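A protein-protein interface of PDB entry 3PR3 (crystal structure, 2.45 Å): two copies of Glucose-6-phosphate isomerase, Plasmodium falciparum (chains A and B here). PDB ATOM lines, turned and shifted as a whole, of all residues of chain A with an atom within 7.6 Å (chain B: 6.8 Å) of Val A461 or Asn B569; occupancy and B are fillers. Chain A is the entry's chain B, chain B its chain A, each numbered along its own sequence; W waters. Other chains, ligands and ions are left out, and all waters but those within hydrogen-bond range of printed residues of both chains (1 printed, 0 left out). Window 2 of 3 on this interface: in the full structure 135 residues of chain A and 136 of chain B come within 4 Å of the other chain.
NE of Arg B262 is in salt-bridge range of OE2 of Glu A460. The backbone carbonyl oxygen (O) of Val A461 is in hydrogen-bond range of the side-chain amide nitrogen (ND2) of Asn B569. The guanidinium group (NE) of Arg B565 is in salt-bridge range of the side-chain carboxylate (OE1) of Glu A467, at 2.9 Å. OD2 of Asp A466 is in salt-bridge range of NE of Arg B572, 2.8 Å away.
No position is printed for both chains.
The backbone carbonyl oxygen (O) of Asn B569 is in hydrogen-bond range of the side-chain amide nitrogen (ND2) of Asn B573 (2.9 Å). The backbone NH (N) of Asp A466 is in hydrogen-bond range of the side-chain hydroxyl (OG) of Ser A463 (3.2 Å). The side-chain amino group of Lys B575 lies within hydrogen-bond range of the side-chain amide oxygen of Asn B569 (2.8 Å). The backbone carbonyl oxygen (O) of Glu A467 lies within hydrogen-bond range of the side-chain hydroxyl (OG1) of Thr A470 (2.7 Å).
Among the printed residues, merely in contact across the chains: Val A462 with Arg B565 (3.7 Å), Val A462 with Phe B568 (3.9 Å), Asp A466 with Phe B568 (3.4 Å), Thr A470 with Val B564 (3.7 Å), Thr A470 with Arg B565 (3.5 Å) and Thr A470 with Phe B568 (3.6 Å).
Water W1 lies within hydrogen-bond range of OE2 of Glu A467 (2.8 Å), OG1 of Thr A470 (3.2 Å) and NH2 of Arg B565 (3.4 Å).
Printed residues of chain B that touch a printed residue of chain A: Arg B262, Val B564, Arg B565, Phe B568, Asn B569 and Arg B572. Hydrophobic or aromatic side chains of chain B that line the printed part of chain A: Val B564 and Phe B568. Along chain B the printed residues that touch a printed residue of chain A span positions 262 to 572. Of the 11 printed residues of chain A, 6 touch a printed residue of chain B. Hydrophobic or aromatic side chains of chain A within 4 Å of the printed part of chain B: Val A461 and Val A462. Among the printed residues, Asp or Glu carboxylates within 4 Å of a Lys or Arg side-chain nitrogen of the other chain: Glu A460 with Arg B262 (2.7 Å), Asp A466 with Arg B572 (2.8 Å) and Glu A467 with Arg B565 (2.9 Å).
Of the printed residues of chain B, Val A461 touches Asn B569. Of chain A, only Val A461 (3.1 Å) comes within 4 Å of Asn B569. Printed residues of chain A within 4 Å of Arg B565: Val A462 (3.7 Å), Glu A467 (2.9 Å) and Thr A470 (3.5 Å). Of the printed residues of chain A, Arg B262 touches Glu A460. Tyr B567 touches none of the printed residues of chain A. Lys B575 touches none of the printed residues of chain A. The nearest residue of chain A that does not touch Asn B569 is Val A462 (4.1 Å). The nearest printed residue of chain A that does not touch Arg B565 is Val A461 (4.02 Å).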
ATOM      1  N   LYS A 456     -12.126  40.803   5.943  1.00  0.00           N
ATOM      2  CA  LYS A 456     -11.677  39.609   5.238  1.00  0.00           C
ATOM      3  C   LYS A 456     -10.401  39.926   4.472  1.00  0.00           C
ATOM      4  O   LYS A 456     -10.324  40.942   3.775  1.00  0.00           O
ATOM      5  CB  LYS A 456     -12.762  39.039   4.303  1.00  0.00           C
ATOM      6  CG  LYS A 456     -12.390  37.680   3.711  1.00  0.00           C
ATOM      7  CD  LYS A 456     -13.620  36.861   3.366  1.00  0.00           C
ATOM      8  CE  LYS A 456     -13.862  36.669   1.893  1.00  0.00           C
ATOM      9  NZ  LYS A 456     -14.727  37.749   1.333  1.00  0.00           N
ATOM     10  N   PHE A 457      -9.404  39.061   4.626  1.00  0.00           N
ATOM     11  CA  PHE A 457      -8.111  39.113   3.935  1.00  0.00           C
ATOM     12  C   PHE A 457      -7.971  37.829   3.112  1.00  0.00           C
ATOM     13  O   PHE A 457      -8.437  36.772   3.546  1.00  0.00           O
ATOM     14  CB  PHE A 457      -6.977  39.268   4.941  1.00  0.00           C
ATOM     15  CG  PHE A 457      -7.086  40.528   5.766  1.00  0.00           C
ATOM     16  CD1 PHE A 457      -7.333  40.461   7.132  1.00  0.00           C
ATOM     17  CD2 PHE A 457      -6.930  41.782   5.179  1.00  0.00           C
ATOM     18  CE1 PHE A 457      -7.416  41.621   7.899  1.00  0.00           C
ATOM     19  CE2 PHE A 457      -7.015  42.943   5.952  1.00  0.00           C
ATOM     20  CZ  PHE A 457      -7.274  42.851   7.303  1.00  0.00           C
ATOM     21  N   ASP A 458      -7.365  37.923   1.913  1.00  0.00           N
ATOM     22  CA  ASP A 458      -7.209  36.784   1.003  1.00  0.00           C
ATOM     23  C   ASP A 458      -6.466  35.570   1.561  1.00  0.00           C
ATOM     24  O   ASP A 458      -6.812  34.442   1.206  1.00  0.00           O
ATOM     25  CB  ASP A 458      -6.684  37.221  -0.368  1.00  0.00           C
ATOM     26  CG  ASP A 458      -7.598  38.235  -1.028  1.00  0.00           C
ATOM     27  OD1 ASP A 458      -8.509  37.816  -1.776  1.00  0.00           O
ATOM     28  OD2 ASP A 458      -7.437  39.440  -0.754  1.00  0.00           O
ATOM     29  N   LYS A 459      -5.480  35.776   2.452  1.00  0.00           N
ATOM     30  CA  LYS A 459      -4.735  34.646   3.033  1.00  0.00           C
ATOM     31  C   LYS A 459      -5.520  33.855   4.108  1.00  0.00           C
ATOM     32  O   LYS A 459      -5.188  32.695   4.394  1.00  0.00           O
ATOM     33  CB  LYS A 459      -3.366  35.105   3.544  1.00  0.00           C
ATOM     34  N   GLU A 460      -6.589  34.468   4.658  1.00  0.00           N
ATOM     35  CA  GLU A 460      -7.428  33.894   5.711  1.00  0.00           C
ATOM     36  C   GLU A 460      -8.391  32.821   5.247  1.00  0.00           C
ATOM     37  O   GLU A 460      -9.047  32.973   4.235  1.00  0.00           O
ATOM     38  CB  GLU A 460      -8.196  35.005   6.463  1.00  0.00           C
ATOM     39  CG  GLU A 460      -7.308  35.978   7.222  1.00  0.00           C
ATOM     40  CD  GLU A 460      -6.488  35.397   8.354  1.00  0.00           C
ATOM     41  OE1 GLU A 460      -6.937  34.403   8.977  1.00  0.00           O
ATOM     42  OE2 GLU A 460      -5.422  35.986   8.655  1.00  0.00           O
ATOM     43  N   VAL A 461      -8.515  31.762   6.037  1.00  0.00           N
ATOM     44  CA  VAL A 461      -9.421  30.634   5.825  1.00  0.00           C
ATOM     45  C   VAL A 461     -10.885  31.175   5.839  1.00  0.00           C
ATOM     46  O   VAL A 461     -11.699  30.784   4.994  1.00  0.00           O
ATOM     47  CB  VAL A 461      -9.157  29.548   6.928  1.00  0.00           C
ATOM     48  CG1 VAL A 461     -10.236  28.464   6.959  1.00  0.00           C
ATOM     49  CG2 VAL A 461      -7.787  28.917   6.773  1.00  0.00           C
ATOM     50  N   VAL A 462     -11.206  32.081   6.787  1.00  0.00           N
ATOM     51  CA  VAL A 462     -12.542  32.691   6.943  1.00  0.00           C
ATOM     52  C   VAL A 462     -12.483  34.198   7.208  1.00  0.00           C
ATOM     53  O   VAL A 462     -11.472  34.721   7.690  1.00  0.00           O
ATOM     54  CB  VAL A 462     -13.446  31.985   8.028  1.00  0.00           C
ATOM     55  CG1 VAL A 462     -13.921  30.603   7.579  1.00  0.00           C
ATOM     56  CG2 VAL A 462     -12.773  31.921   9.396  1.00  0.00           C
ATOM     57  N   SER A 463     -13.616  34.886   6.955  1.00  0.00           N
ATOM     58  CA  SER A 463     -13.796  36.303   7.304  1.00  0.00           C
ATOM     59  C   SER A 463     -13.796  36.383   8.859  1.00  0.00           C
ATOM     60  O   SER A 463     -14.155  35.406   9.514  1.00  0.00           O
ATOM     61  CB  SER A 463     -15.128  36.810   6.769  1.00  0.00           C
ATOM     62  OG  SER A 463     -16.210  36.158   7.417  1.00  0.00           O
ATOM     63  N   ASP A 466     -17.070  35.402  10.363  1.00  0.00           N
ATOM     64  CA  ASP A 466     -17.291  33.960  10.319  1.00  0.00           C
ATOM     65  C   ASP A 466     -16.523  33.292  11.425  1.00  0.00           C
ATOM     66  O   ASP A 466     -17.058  32.381  12.058  1.00  0.00           O
ATOM     67  CB  ASP A 466     -16.895  33.360   8.953  1.00  0.00           C
ATOM     68  CG  ASP A 466     -17.970  33.427   7.863  1.00  0.00           C
ATOM     69  OD1 ASP A 466     -19.073  33.965   8.137  1.00  0.00           O
ATOM     70  OD2 ASP A 466     -17.709  32.943   6.741  1.00  0.00           O
ATOM     71  N   GLU A 467     -15.286  33.772  11.700  1.00  0.00           N
ATOM     72  CA  GLU A 467     -14.450  33.210  12.774  1.00  0.00           C
ATOM     73  C   GLU A 467     -15.175  33.311  14.119  1.00  0.00           C
ATOM     74  O   GLU A 467     -15.244  32.328  14.862  1.00  0.00           O
ATOM     75  CB  GLU A 467     -13.065  33.872  12.827  1.00  0.00           C
ATOM     76  CG  GLU A 467     -12.115  33.250  13.848  1.00  0.00           C
ATOM     77  CD  GLU A 467     -11.844  31.760  13.743  1.00  0.00           C
ATOM     78  OE1 GLU A 467     -11.790  31.229  12.611  1.00  0.00           O
ATOM     79  OE2 GLU A 467     -11.642  31.128  14.803  1.00  0.00           O
ATOM     80  N   THR A 470     -18.225  30.807  14.273  1.00  0.00           N
ATOM     81  CA  THR A 470     -17.912  29.374  14.445  1.00  0.00           C
ATOM     82  C   THR A 470     -18.190  28.976  15.894  1.00  0.00           C
ATOM     83  O   THR A 470     -18.724  27.900  16.156  1.00  0.00           O
ATOM     84  CB  THR A 470     -16.458  29.031  14.027  1.00  0.00           C
ATOM     85  OG1 THR A 470     -15.511  29.664  14.894  1.00  0.00           O
ATOM     86  CG2 THR A 470     -16.165  29.385  12.607  1.00  0.00           C
ATOM     87  N   ARG B 262      -2.853  39.448  13.140  1.00  0.00           N
ATOM     88  CA  ARG B 262      -2.640  39.485  11.685  1.00  0.00           C
ATOM     89  C   ARG B 262      -3.391  40.643  11.051  1.00  0.00           C
ATOM     90  O   ARG B 262      -2.860  41.275  10.140  1.00  0.00           O
ATOM     91  CB  ARG B 262      -3.027  38.151  10.998  1.00  0.00           C
ATOM     92  CG  ARG B 262      -2.196  36.972  11.485  1.00  0.00           C
ATOM     93  CD  ARG B 262      -2.392  35.708  10.658  1.00  0.00           C
ATOM     94  NE  ARG B 262      -3.767  35.199  10.637  1.00  0.00           N
ATOM     95  CZ  ARG B 262      -4.272  34.346  11.525  1.00  0.00           C
ATOM     96  NH1 ARG B 262      -3.542  33.940  12.556  1.00  0.00           N
ATOM     97  NH2 ARG B 262      -5.522  33.915  11.406  1.00  0.00           N
ATOM     98  N   VAL B 564     -16.683  23.904  12.509  1.00  0.00           N
ATOM     99  CA  VAL B 564     -17.551  24.916  11.902  1.00  0.00           C
ATOM    100  C   VAL B 564     -16.741  25.830  10.964  1.00  0.00           C
ATOM    101  O   VAL B 564     -17.240  26.173   9.884  1.00  0.00           O
ATOM    102  CB  VAL B 564     -18.383  25.715  12.942  1.00  0.00           C
ATOM    103  CG1 VAL B 564     -19.301  26.742  12.253  1.00  0.00           C
ATOM    104  CG2 VAL B 564     -19.202  24.770  13.828  1.00  0.00           C
ATOM    105  N   ARG B 565     -15.494  26.200  11.358  1.00  0.00           N
ATOM    106  CA  ARG B 565     -14.606  27.043  10.547  1.00  0.00           C
ATOM    107  C   ARG B 565     -14.349  26.392   9.181  1.00  0.00           C
ATOM    108  O   ARG B 565     -14.568  27.032   8.149  1.00  0.00           O
ATOM    109  CB  ARG B 565     -13.286  27.323  11.270  1.00  0.00           C
ATOM    110  CG  ARG B 565     -12.339  28.205  10.464  1.00  0.00           C
ATOM    111  CD  ARG B 565     -10.910  28.001  10.898  1.00  0.00           C
ATOM    112  NE  ARG B 565     -10.631  28.627  12.192  1.00  0.00           N
ATOM    113  CZ  ARG B 565      -9.676  28.229  13.028  1.00  0.00           C
ATOM    114  NH1 ARG B 565      -8.916  27.180  12.730  1.00  0.00           N
ATOM    115  NH2 ARG B 565      -9.480  28.869  14.176  1.00  0.00           N
ATOM    116  N   ASN B 566     -13.921  25.110   9.197  1.00  0.00           N
ATOM    117  CA  ASN B 566     -13.683  24.291   8.007  1.00  0.00           C
ATOM    118  C   ASN B 566     -14.941  24.205   7.147  1.00  0.00           C
ATOM    119  O   ASN B 566     -14.847  24.405   5.938  1.00  0.00           O
ATOM    120  CB  ASN B 566     -13.206  22.881   8.404  1.00  0.00           C
ATOM    121  CG  ASN B 566     -11.822  22.896   8.987  1.00  0.00           C
ATOM    122  OD1 ASN B 566     -10.988  23.743   8.643  1.00  0.00           O
ATOM    123  ND2 ASN B 566     -11.558  21.989   9.913  1.00  0.00           N
ATOM    124  N   TYR B 567     -16.120  23.963   7.785  1.00  0.00           N
ATOM    125  CA  TYR B 567     -17.412  23.897   7.108  1.00  0.00           C
ATOM    126  C   TYR B 567     -17.706  25.211   6.412  1.00  0.00           C
ATOM    127  O   TYR B 567     -18.134  25.201   5.259  1.00  0.00           O
ATOM    128  CB  TYR B 567     -18.542  23.515   8.087  1.00  0.00           C
ATOM    129  CG  TYR B 567     -19.900  23.449   7.417  1.00  0.00           C
ATOM    130  CD1 TYR B 567     -20.248  22.371   6.606  1.00  0.00           C
ATOM    131  CD2 TYR B 567     -20.822  24.484   7.557  1.00  0.00           C
ATOM    132  CE1 TYR B 567     -21.478  22.326   5.950  1.00  0.00           C
ATOM    133  CE2 TYR B 567     -22.050  24.454   6.896  1.00  0.00           C
ATOM    134  CZ  TYR B 567     -22.378  23.370   6.098  1.00  0.00           C
ATOM    135  OH  TYR B 567     -23.603  23.306   5.469  1.00  0.00           O
ATOM    136  N   PHE B 568     -17.458  26.352   7.108  1.00  0.00           N
ATOM    137  CA  PHE B 568     -17.676  27.697   6.545  1.00  0.00           C
ATOM    138  C   PHE B 568     -16.768  27.915   5.351  1.00  0.00           C
ATOM    139  O   PHE B 568     -17.215  28.455   4.352  1.00  0.00           O
ATOM    140  CB  PHE B 568     -17.427  28.803   7.582  1.00  0.00           C
ATOM    141  CG  PHE B 568     -18.504  29.091   8.611  1.00  0.00           C
ATOM    142  CD1 PHE B 568     -18.257  29.949   9.678  1.00  0.00           C
ATOM    143  CD2 PHE B 568     -19.764  28.519   8.507  1.00  0.00           C
ATOM    144  CE1 PHE B 568     -19.253  30.232  10.619  1.00  0.00           C
ATOM    145  CE2 PHE B 568     -20.757  28.790   9.459  1.00  0.00           C
ATOM    146  CZ  PHE B 568     -20.491  29.642  10.510  1.00  0.00           C
ATOM    147  N   ASN B 569     -15.518  27.468   5.427  1.00  0.00           N
ATOM    148  CA  ASN B 569     -14.581  27.610   4.315  1.00  0.00           C
ATOM    149  C   ASN B 569     -15.021  26.771   3.091  1.00  0.00           C
ATOM    150  O   ASN B 569     -15.097  27.295   1.983  1.00  0.00           O
ATOM    151  CB  ASN B 569     -13.166  27.338   4.787  1.00  0.00           C
ATOM    152  CG  ASN B 569     -12.170  27.248   3.669  1.00  0.00           C
ATOM    153  OD1 ASN B 569     -11.814  26.164   3.280  1.00  0.00           O
ATOM    154  ND2 ASN B 569     -11.743  28.363   3.082  1.00  0.00           N
ATOM    155  N   ASP B 570     -15.441  25.525   3.327  1.00  0.00           N
ATOM    156  CA  ASP B 570     -15.997  24.638   2.296  1.00  0.00           C
ATOM    157  C   ASP B 570     -17.242  25.242   1.675  1.00  0.00           C
ATOM    158  O   ASP B 570     -17.273  25.401   0.461  1.00  0.00           O
ATOM    159  CB  ASP B 570     -16.340  23.251   2.868  1.00  0.00           C
ATOM    160  CG  ASP B 570     -15.138  22.396   3.128  1.00  0.00           C
ATOM    161  OD1 ASP B 570     -14.026  22.816   2.767  1.00  0.00           O
ATOM    162  OD2 ASP B 570     -15.302  21.317   3.704  1.00  0.00           O
ATOM    163  N   THR B 571     -18.234  25.632   2.505  1.00  0.00           N
ATOM    164  CA  THR B 571     -19.518  26.187   2.043  1.00  0.00           C
ATOM    165  C   THR B 571     -19.426  27.523   1.280  1.00  0.00           C
ATOM    166  O   THR B 571     -19.985  27.627   0.185  1.00  0.00           O
ATOM    167  CB  THR B 571     -20.594  26.146   3.148  1.00  0.00           C
ATOM    168  OG1 THR B 571     -20.478  24.935   3.898  1.00  0.00           O
ATOM    169  CG2 THR B 571     -22.000  26.216   2.583  1.00  0.00           C
ATOM    170  N   ARG B 572     -18.726  28.524   1.851  1.00  0.00           N
ATOM    171  CA  ARG B 572     -18.539  29.863   1.254  1.00  0.00           C
ATOM    172  C   ARG B 572     -17.831  29.790  -0.091  1.00  0.00           C
ATOM    173  O   ARG B 572     -18.113  30.598  -0.975  1.00  0.00           O
ATOM    174  CB  ARG B 572     -17.753  30.808   2.199  1.00  0.00           C
ATOM    175  CG  ARG B 572     -18.498  31.184   3.485  1.00  0.00           C
ATOM    176  CD  ARG B 572     -19.210  32.508   3.407  1.00  0.00           C
ATOM    177  NE  ARG B 572     -19.659  32.941   4.728  1.00  0.00           N
ATOM    178  CZ  ARG B 572     -20.856  33.453   4.993  1.00  0.00           C
ATOM    179  NH1 ARG B 572     -21.760  33.585   4.026  1.00  0.00           N
ATOM    180  NH2 ARG B 572     -21.160  33.834   6.222  1.00  0.00           N
ATOM    181  N   ASN B 573     -16.906  28.824  -0.233  1.00  0.00           N
ATOM    182  CA  ASN B 573     -16.128  28.606  -1.448  1.00  0.00           C
ATOM    183  C   ASN B 573     -16.723  27.553  -2.389  1.00  0.00           C
ATOM    184  O   ASN B 573     -16.045  27.119  -3.323  1.00  0.00           O
ATOM    185  CB  ASN B 573     -14.664  28.306  -1.104  1.00  0.00           C
ATOM    186  CG  ASN B 573     -13.934  29.511  -0.549  1.00  0.00           C
ATOM    187  OD1 ASN B 573     -13.750  30.530  -1.237  1.00  0.00           O
ATOM    188  ND2 ASN B 573     -13.514  29.429   0.714  1.00  0.00           N
ATOM    189  N   GLN B 574     -17.997  27.162  -2.151  1.00  0.00           N
ATOM    190  CA  GLN B 574     -18.789  26.207  -2.951  1.00  0.00           C
ATOM    191  C   GLN B 574     -17.986  24.940  -3.287  1.00  0.00           C
ATOM    192  O   GLN B 574     -17.958  24.508  -4.446  1.00  0.00           O
ATOM    193  CB  GLN B 574     -19.317  26.859  -4.264  1.00  0.00           C
ATOM    194  CG  GLN B 574     -19.569  28.374  -4.272  1.00  0.00           C
ATOM    195  CD  GLN B 574     -21.013  28.753  -4.066  1.00  0.00           C
ATOM    196  OE1 GLN B 574     -21.936  28.030  -4.690  1.00  0.00           O
ATOM    197  NE2 GLN B 574     -21.315  29.715  -3.350  1.00  0.00           N
ATOM    198  N   LYS B 575     -17.309  24.368  -2.280  1.00  0.00           N
ATOM    199  CA  LYS B 575     -16.463  23.199  -2.469  1.00  0.00           C
ATOM    200  C   LYS B 575     -16.473  22.239  -1.275  1.00  0.00           C
ATOM    201  O   LYS B 575     -17.139  22.513  -0.283  1.00  0.00           O
ATOM    202  CB  LYS B 575     -15.044  23.642  -2.927  1.00  0.00           C
ATOM    203  CG  LYS B 575     -13.889  23.556  -1.936  1.00  0.00           C
ATOM    204  CD  LYS B 575     -13.753  24.732  -1.021  1.00  0.00           C
ATOM    205  CE  LYS B 575     -12.847  24.341   0.122  1.00  0.00           C
ATOM    206  NZ  LYS B 575     -12.051  25.487   0.604  1.00  0.00           N
ATOM    207  N   SER B 577     -13.781  19.146   0.985  1.00  0.00           N
ATOM    208  CA  SER B 577     -12.415  18.956   1.502  1.00  0.00           C
ATOM    209  C   SER B 577     -12.300  17.592   2.217  1.00  0.00           C
ATOM    210  O   SER B 577     -13.296  16.864   2.281  1.00  0.00           O
ATOM    211  CB  SER B 577     -12.037  20.089   2.460  1.00  0.00           C
ATOM    212  OG  SER B 577     -12.846  20.073   3.624  1.00  0.00           O
ATOM    213  N   TYR B 581     -18.378  16.245   8.050  1.00  0.00           N
ATOM    214  CA  TYR B 581     -19.181  16.899   9.081  1.00  0.00           C
ATOM    215  C   TYR B 581     -20.394  16.122   9.505  1.00  0.00           C
ATOM    216  O   TYR B 581     -21.139  15.611   8.664  1.00  0.00           O
ATOM    217  CB  TYR B 581     -19.592  18.313   8.646  1.00  0.00           C
ATOM    218  CG  TYR B 581     -18.456  19.096   8.027  1.00  0.00           C
ATOM    219  CD1 TYR B 581     -17.516  19.746   8.823  1.00  0.00           C
ATOM    220  CD2 TYR B 581     -18.281  19.133   6.641  1.00  0.00           C
ATOM    221  CE1 TYR B 581     -16.429  20.413   8.258  1.00  0.00           C
ATOM    222  CE2 TYR B 581     -17.205  19.803   6.068  1.00  0.00           C
ATOM    223  CZ  TYR B 581     -16.286  20.445   6.881  1.00  0.00           C
ATOM    224  OH  TYR B 581     -15.247  21.133   6.324  1.00  0.00           O
HETATM  225  O   HOH W   1     -12.576  28.576  15.458  1.00  0.00           O
